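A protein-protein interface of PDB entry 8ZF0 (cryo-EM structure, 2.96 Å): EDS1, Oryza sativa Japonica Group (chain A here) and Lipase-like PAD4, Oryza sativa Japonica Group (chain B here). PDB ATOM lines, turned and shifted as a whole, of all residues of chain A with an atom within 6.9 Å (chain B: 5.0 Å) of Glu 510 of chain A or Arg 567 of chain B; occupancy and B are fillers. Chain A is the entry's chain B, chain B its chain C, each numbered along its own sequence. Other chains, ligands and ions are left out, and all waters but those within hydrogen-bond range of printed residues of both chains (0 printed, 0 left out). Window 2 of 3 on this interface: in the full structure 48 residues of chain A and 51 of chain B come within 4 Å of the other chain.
The side-chain amino group of Lys 569 of chain B sits at hydrogen-bond distance from the side-chain hydroxyl of Ser 507 of chain A (3.3 Å).
The side-chain hydroxyl of Ser 568 of chain B lies within hydrogen-bond range of the side-chain carboxylate of Glu 510 of chain A (3.1 Å).
The guanidinium group of Arg 567 of chain B is in salt-bridge range of the side-chain carboxylate of Asp 511 of chain A, 3.7 Å away.
The backbone carbonyl oxygen (O) of Glu 624 of chain B lies within hydrogen-bond range of the backbone NH (N) of Gln 575 of chain B (3.4 Å).
Among the printed residues, pairs that only touch across the chains: Glu 510 of chain A with Arg 567 of chain B (3.8 Å), Glu 510 of chain A with Lys 569 of chain B (3.3 Å), Asp 511 of chain A with Gln 575 of chain B (3.98 Å) and Asn 560 of chain A with Ser 568 of chain B (3.9 Å).
Lys 508 of chain A touches none of the printed residues of chain B.
Of chain B, only Arg 567 (3.8 Å), Ser 568 (3.1 Å) and Lys 569 (3.3 Å) come within 4 Å of Glu 510 of chain A.
Of the printed residues of chain B, Asp 511 of chain A touches Arg 567 and Gln 575.
Printed residues of chain B within 4 Å of Asn 560 of chain A: Ser 568.
Arg 567 of chain B touches just these residues of chain A: Glu 510 and Asp 511.
Of the printed residues of chain A, Ser 568 of chain B touches Glu 510 and Asn 560.
Printed residues of chain A within 4 Å of Lys 569 of chain B: Ser 507 and Glu 510.
The nearest residue of chain B that does not touch Glu 510 of chain A is Arg 566 of chain B (4.9 Å).
The nearest printed residue of chain A that does not touch Gln 575 of chain B is Ser 507 of chain A (6.8 Å).
Of the 11 printed residues of chain A, 4 touch a printed residue of chain B.
Printed residues of chain A that touch a printed residue of chain B: Ser 507, Glu 510, Asp 511 and Asn 560.
Along chain A the printed residues that touch a printed residue of chain B span positions 507 to 560.
Among the printed residues, 7 pairs touch across the chains.
Among the printed residues, Asp or Glu carboxylates within 4 Å of a Lys or Arg side-chain nitrogen of the other chain: Asp 511 of chain A with Arg 567 of chain B (3.7 Å).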
ATOM      1  N   TYR A 503      31.263  25.472  18.576  1.00  0.00           N
ATOM      2  CA  TYR A 503      30.774  24.129  18.285  1.00  0.00           C
ATOM      3  C   TYR A 503      29.399  23.890  18.897  1.00  0.00           C
ATOM      4  O   TYR A 503      28.528  23.281  18.265  1.00  0.00           O
ATOM      5  CB  TYR A 503      31.773  23.088  18.791  1.00  0.00           C
ATOM      6  CG  TYR A 503      31.498  21.683  18.308  1.00  0.00           C
ATOM      7  CD1 TYR A 503      31.786  21.305  17.004  1.00  0.00           C
ATOM      8  CD2 TYR A 503      30.951  20.732  19.160  1.00  0.00           C
ATOM      9  CE1 TYR A 503      31.537  20.020  16.561  1.00  0.00           C
ATOM     10  CE2 TYR A 503      30.698  19.445  18.725  1.00  0.00           C
ATOM     11  CZ  TYR A 503      30.993  19.095  17.426  1.00  0.00           C
ATOM     12  OH  TYR A 503      30.742  17.815  16.989  1.00  0.00           O
ATOM     13  N   HIS A 506      26.142  26.263  17.604  1.00  0.00           N
ATOM     14  CA  HIS A 506      25.560  25.895  16.322  1.00  0.00           C
ATOM     15  C   HIS A 506      24.857  24.546  16.369  1.00  0.00           C
ATOM     16  O   HIS A 506      24.440  24.041  15.321  1.00  0.00           O
ATOM     17  CB  HIS A 506      26.637  25.887  15.236  1.00  0.00           C
ATOM     18  CG  HIS A 506      26.995  27.249  14.729  1.00  0.00           C
ATOM     19  ND1 HIS A 506      28.286  27.730  14.735  1.00  0.00           N
ATOM     20  CD2 HIS A 506      26.230  28.233  14.201  1.00  0.00           C
ATOM     21  CE1 HIS A 506      28.302  28.952  14.232  1.00  0.00           C
ATOM     22  NE2 HIS A 506      27.066  29.281  13.901  1.00  0.00           N
ATOM     23  N   SER A 507      24.717  23.956  17.559  1.00  0.00           N
ATOM     24  CA  SER A 507      24.082  22.649  17.736  1.00  0.00           C
ATOM     25  C   SER A 507      24.766  21.578  16.890  1.00  0.00           C
ATOM     26  O   SER A 507      24.113  20.722  16.290  1.00  0.00           O
ATOM     27  CB  SER A 507      22.584  22.714  17.425  1.00  0.00           C
ATOM     28  OG  SER A 507      21.907  23.541  18.355  1.00  0.00           O
ATOM     29  N   LYS A 508      26.096  21.626  16.842  1.00  0.00           N
ATOM     30  CA  LYS A 508      26.874  20.645  16.095  1.00  0.00           C
ATOM     31  C   LYS A 508      27.126  19.365  16.879  1.00  0.00           C
ATOM     32  O   LYS A 508      27.696  18.420  16.323  1.00  0.00           O
ATOM     33  CB  LYS A 508      28.210  21.251  15.660  1.00  0.00           C
ATOM     34  CG  LYS A 508      28.074  22.487  14.791  1.00  0.00           C
ATOM     35  CD  LYS A 508      29.389  22.833  14.117  1.00  0.00           C
ATOM     36  CE  LYS A 508      29.169  23.747  12.924  1.00  0.00           C
ATOM     37  NZ  LYS A 508      28.052  23.271  12.062  1.00  0.00           N
ATOM     38  N   ASN A 509      26.724  19.310  18.148  1.00  0.00           N
ATOM     39  CA  ASN A 509      26.904  18.116  18.961  1.00  0.00           C
ATOM     40  C   ASN A 509      25.762  17.121  18.822  1.00  0.00           C
ATOM     41  O   ASN A 509      25.853  16.018  19.371  1.00  0.00           O
ATOM     42  CB  ASN A 509      27.063  18.502  20.436  1.00  0.00           C
ATOM     43  CG  ASN A 509      25.886  19.299  20.960  1.00  0.00           C
ATOM     44  OD1 ASN A 509      25.559  20.363  20.436  1.00  0.00           O
ATOM     45  ND2 ASN A 509      25.241  18.786  22.000  1.00  0.00           N
ATOM     46  N   GLU A 510      24.695  17.477  18.108  1.00  0.00           N
ATOM     47  CA  GLU A 510      23.545  16.599  17.942  1.00  0.00           C
ATOM     48  C   GLU A 510      23.502  15.911  16.584  1.00  0.00           C
ATOM     49  O   GLU A 510      22.680  15.008  16.394  1.00  0.00           O
ATOM     50  CB  GLU A 510      22.245  17.385  18.153  1.00  0.00           C
ATOM     51  CG  GLU A 510      22.105  17.983  19.543  1.00  0.00           C
ATOM     52  CD  GLU A 510      20.720  18.543  19.800  1.00  0.00           C
ATOM     53  OE1 GLU A 510      20.293  19.442  19.046  1.00  0.00           O
ATOM     54  OE2 GLU A 510      20.060  18.085  20.755  1.00  0.00           O
ATOM     55  N   ASP A 511      24.360  16.307  15.643  1.00  0.00           N
ATOM     56  CA  ASP A 511      24.417  15.673  14.334  1.00  0.00           C
ATOM     57  C   ASP A 511      25.744  14.995  14.035  1.00  0.00           C
ATOM     58  O   ASP A 511      25.791  14.148  13.135  1.00  0.00           O
ATOM     59  CB  ASP A 511      24.127  16.697  13.224  1.00  0.00           C
ATOM     60  CG  ASP A 511      24.774  18.040  13.486  1.00  0.00           C
ATOM     61  OD1 ASP A 511      25.584  18.134  14.431  1.00  0.00           O
ATOM     62  OD2 ASP A 511      24.476  19.001  12.747  1.00  0.00           O
ATOM     63  N   THR A 512      26.815  15.336  14.750  1.00  0.00           N
ATOM     64  CA  THR A 512      28.121  14.719  14.557  1.00  0.00           C
ATOM     65  C   THR A 512      28.568  13.904  15.762  1.00  0.00           C
ATOM     66  O   THR A 512      28.896  12.721  15.621  1.00  0.00           O
ATOM     67  CB  THR A 512      29.172  15.795  14.243  1.00  0.00           C
ATOM     68  OG1 THR A 512      28.838  16.445  13.010  1.00  0.00           O
ATOM     69  CG2 THR A 512      30.554  15.170  14.121  1.00  0.00           C
ATOM     70  N   GLY A 513      28.586  14.502  16.940  1.00  0.00           N
ATOM     71  CA  GLY A 513      28.984  13.805  18.143  1.00  0.00           C
ATOM     72  C   GLY A 513      29.549  14.779  19.157  1.00  0.00           C
ATOM     73  O   GLY A 513      29.490  15.993  18.981  1.00  0.00           O
ATOM     74  N   SER A 514      30.101  14.215  20.227  1.00  0.00           N
ATOM     75  CA  SER A 514      30.698  15.022  21.278  1.00  0.00           C
ATOM     76  C   SER A 514      31.956  15.722  20.775  1.00  0.00           C
ATOM     77  O   SER A 514      32.648  15.235  19.876  1.00  0.00           O
ATOM     78  CB  SER A 514      31.031  14.157  22.494  1.00  0.00           C
ATOM     79  OG  SER A 514      31.906  14.835  23.378  1.00  0.00           O
ATOM     80  N   ASN A 560      18.648  15.403  29.120  1.00  0.00           N
ATOM     81  CA  ASN A 560      18.152  14.485  28.102  1.00  0.00           C
ATOM     82  C   ASN A 560      17.412  13.295  28.703  1.00  0.00           C
ATOM     83  O   ASN A 560      17.132  12.323  27.995  1.00  0.00           O
ATOM     84  CB  ASN A 560      19.303  14.001  27.218  1.00  0.00           C
ATOM     85  CG  ASN A 560      19.674  15.003  26.144  1.00  0.00           C
ATOM     86  OD1 ASN A 560      19.061  16.066  26.031  1.00  0.00           O
ATOM     87  ND2 ASN A 560      20.681  14.670  25.345  1.00  0.00           N
ATOM     88  N   ALA B 565      20.349   9.338  19.158  1.00  0.00           N
ATOM     89  CA  ALA B 565      19.419   9.941  20.101  1.00  0.00           C
ATOM     90  C   ALA B 565      18.601  11.031  19.421  1.00  0.00           C
ATOM     91  O   ALA B 565      19.082  11.722  18.520  1.00  0.00           O
ATOM     92  CB  ALA B 565      20.176  10.518  21.299  1.00  0.00           C
ATOM     93  N   ARG B 566      17.351  11.176  19.856  1.00  0.00           N
ATOM     94  CA  ARG B 566      16.473  12.185  19.281  1.00  0.00           C
ATOM     95  C   ARG B 566      16.990  13.584  19.592  1.00  0.00           C
ATOM     96  O   ARG B 566      17.543  13.845  20.665  1.00  0.00           O
ATOM     97  CB  ARG B 566      15.050  12.021  19.814  1.00  0.00           C
ATOM     98  CG  ARG B 566      14.561  10.583  19.853  1.00  0.00           C
ATOM     99  CD  ARG B 566      13.547  10.370  20.973  1.00  0.00           C
ATOM    100  NE  ARG B 566      13.944  10.995  22.231  1.00  0.00           N
ATOM    101  CZ  ARG B 566      15.003  10.650  22.953  1.00  0.00           C
ATOM    102  NH1 ARG B 566      15.794   9.652  22.591  1.00  0.00           N
ATOM    103  NH2 ARG B 566      15.270  11.317  24.071  1.00  0.00           N
ATOM    104  N   ARG B 567      16.804  14.491  18.637  1.00  0.00           N
ATOM    105  CA  ARG B 567      17.241  15.872  18.798  1.00  0.00           C
ATOM    106  C   ARG B 567      16.284  16.600  19.734  1.00  0.00           C
ATOM    107  O   ARG B 567      15.097  16.748  19.426  1.00  0.00           O
ATOM    108  CB  ARG B 567      17.310  16.568  17.442  1.00  0.00           C
ATOM    109  CG  ARG B 567      17.945  15.728  16.346  1.00  0.00           C
ATOM    110  CD  ARG B 567      18.142  16.535  15.074  1.00  0.00           C
ATOM    111  NE  ARG B 567      19.252  17.474  15.186  1.00  0.00           N
ATOM    112  CZ  ARG B 567      20.329  17.454  14.413  1.00  0.00           C
ATOM    113  NH1 ARG B 567      20.477  16.552  13.456  1.00  0.00           N
ATOM    114  NH2 ARG B 567      21.283  18.361  14.605  1.00  0.00           N
ATOM    115  N   SER B 568      16.801  17.055  20.878  1.00  0.00           N
ATOM    116  CA  SER B 568      15.980  17.776  21.842  1.00  0.00           C
ATOM    117  C   SER B 568      15.639  19.188  21.389  1.00  0.00           C
ATOM    118  O   SER B 568      14.777  19.826  22.004  1.00  0.00           O
ATOM    119  CB  SER B 568      16.688  17.826  23.197  1.00  0.00           C
ATOM    120  OG  SER B 568      18.001  18.343  23.066  1.00  0.00           O
ATOM    121  N   LYS B 569      16.285  19.689  20.339  1.00  0.00           N
ATOM    122  CA  LYS B 569      16.015  21.026  19.835  1.00  0.00           C
ATOM    123  C   LYS B 569      16.211  21.031  18.328  1.00  0.00           C
ATOM    124  O   LYS B 569      16.857  20.145  17.762  1.00  0.00           O
ATOM    125  CB  LYS B 569      16.920  22.073  20.496  1.00  0.00           C
ATOM    126  CG  LYS B 569      18.366  21.631  20.653  1.00  0.00           C
ATOM    127  CD  LYS B 569      19.238  22.764  21.167  1.00  0.00           C
ATOM    128  CE  LYS B 569      20.674  22.308  21.363  1.00  0.00           C
ATOM    129  NZ  LYS B 569      21.580  23.446  21.678  1.00  0.00           N
ATOM    130  N   ALA B 571      17.666  21.798  14.782  1.00  0.00           N
ATOM    131  CA  ALA B 571      19.039  21.953  14.330  1.00  0.00           C
ATOM    132  C   ALA B 571      19.283  23.368  13.819  1.00  0.00           C
ATOM    133  O   ALA B 571      18.366  24.057  13.363  1.00  0.00           O
ATOM    134  CB  ALA B 571      19.359  20.938  13.232  1.00  0.00           C
ATOM    135  N   GLN B 575      19.265  19.803   7.430  1.00  0.00           N
ATOM    136  CA  GLN B 575      20.135  18.731   6.956  1.00  0.00           C
ATOM    137  C   GLN B 575      20.022  18.546   5.447  1.00  0.00           C
ATOM    138  O   GLN B 575      21.023  18.277   4.774  1.00  0.00           O
ATOM    139  CB  GLN B 575      19.810  17.430   7.687  1.00  0.00           C
ATOM    140  CG  GLN B 575      20.032  17.498   9.189  1.00  0.00           C
ATOM    141  CD  GLN B 575      21.385  18.080   9.551  1.00  0.00           C
ATOM    142  OE1 GLN B 575      22.426  17.528   9.195  1.00  0.00           O
ATOM    143  NE2 GLN B 575      21.376  19.201  10.261  1.00  0.00           N
ATOM    144  N   ASN B 622      11.467  14.415  13.530  1.00  0.00           N
ATOM    145  CA  ASN B 622      12.822  14.198  14.020  1.00  0.00           C
ATOM    146  C   ASN B 622      13.552  15.496  14.336  1.00  0.00           C
ATOM    147  O   ASN B 622      14.689  15.442  14.819  1.00  0.00           O
ATOM    148  CB  ASN B 622      13.628  13.387  13.000  1.00  0.00           C
ATOM    149  CG  ASN B 622      12.838  12.232  12.419  1.00  0.00           C
ATOM    150  OD1 ASN B 622      11.940  11.692  13.064  1.00  0.00           O
ATOM    151  ND2 ASN B 622      13.170  11.848  11.193  1.00  0.00           N
ATOM    152  N   LYS B 623      12.931  16.648  14.073  1.00  0.00           N
ATOM    153  CA  LYS B 623      13.527  17.959  14.338  1.00  0.00           C
ATOM    154  C   LYS B 623      14.856  18.126  13.605  1.00  0.00           C
ATOM    155  O   LYS B 623      15.813  18.694  14.135  1.00  0.00           O
ATOM    156  CB  LYS B 623      13.700  18.197  15.841  1.00  0.00           C
ATOM    157  CG  LYS B 623      12.394  18.226  16.616  1.00  0.00           C
ATOM    158  CD  LYS B 623      12.631  18.521  18.087  1.00  0.00           C
ATOM    159  CE  LYS B 623      11.338  18.437  18.882  1.00  0.00           C
ATOM    160  NZ  LYS B 623      11.553  18.740  20.324  1.00  0.00           N
ATOM    161  N   GLU B 624      14.915  17.628  12.373  1.00  0.00           N
ATOM    162  CA  GLU B 624      16.094  17.774  11.531  1.00  0.00           C
ATOM    163  C   GLU B 624      16.084  19.064  10.722  1.00  0.00           C
ATOM    164  O   GLU B 624      17.032  19.314   9.971  1.00  0.00           O
ATOM    165  CB  GLU B 624      16.220  16.575  10.585  1.00  0.00           C
ATOM    166  CG  GLU B 624      16.450  15.251  11.293  1.00  0.00           C
ATOM    167  CD  GLU B 624      16.670  14.104  10.326  1.00  0.00           C
ATOM    168  OE1 GLU B 624      17.634  14.168   9.536  1.00  0.00           O
ATOM    169  OE2 GLU B 624      15.878  13.139  10.358  1.00  0.00           O
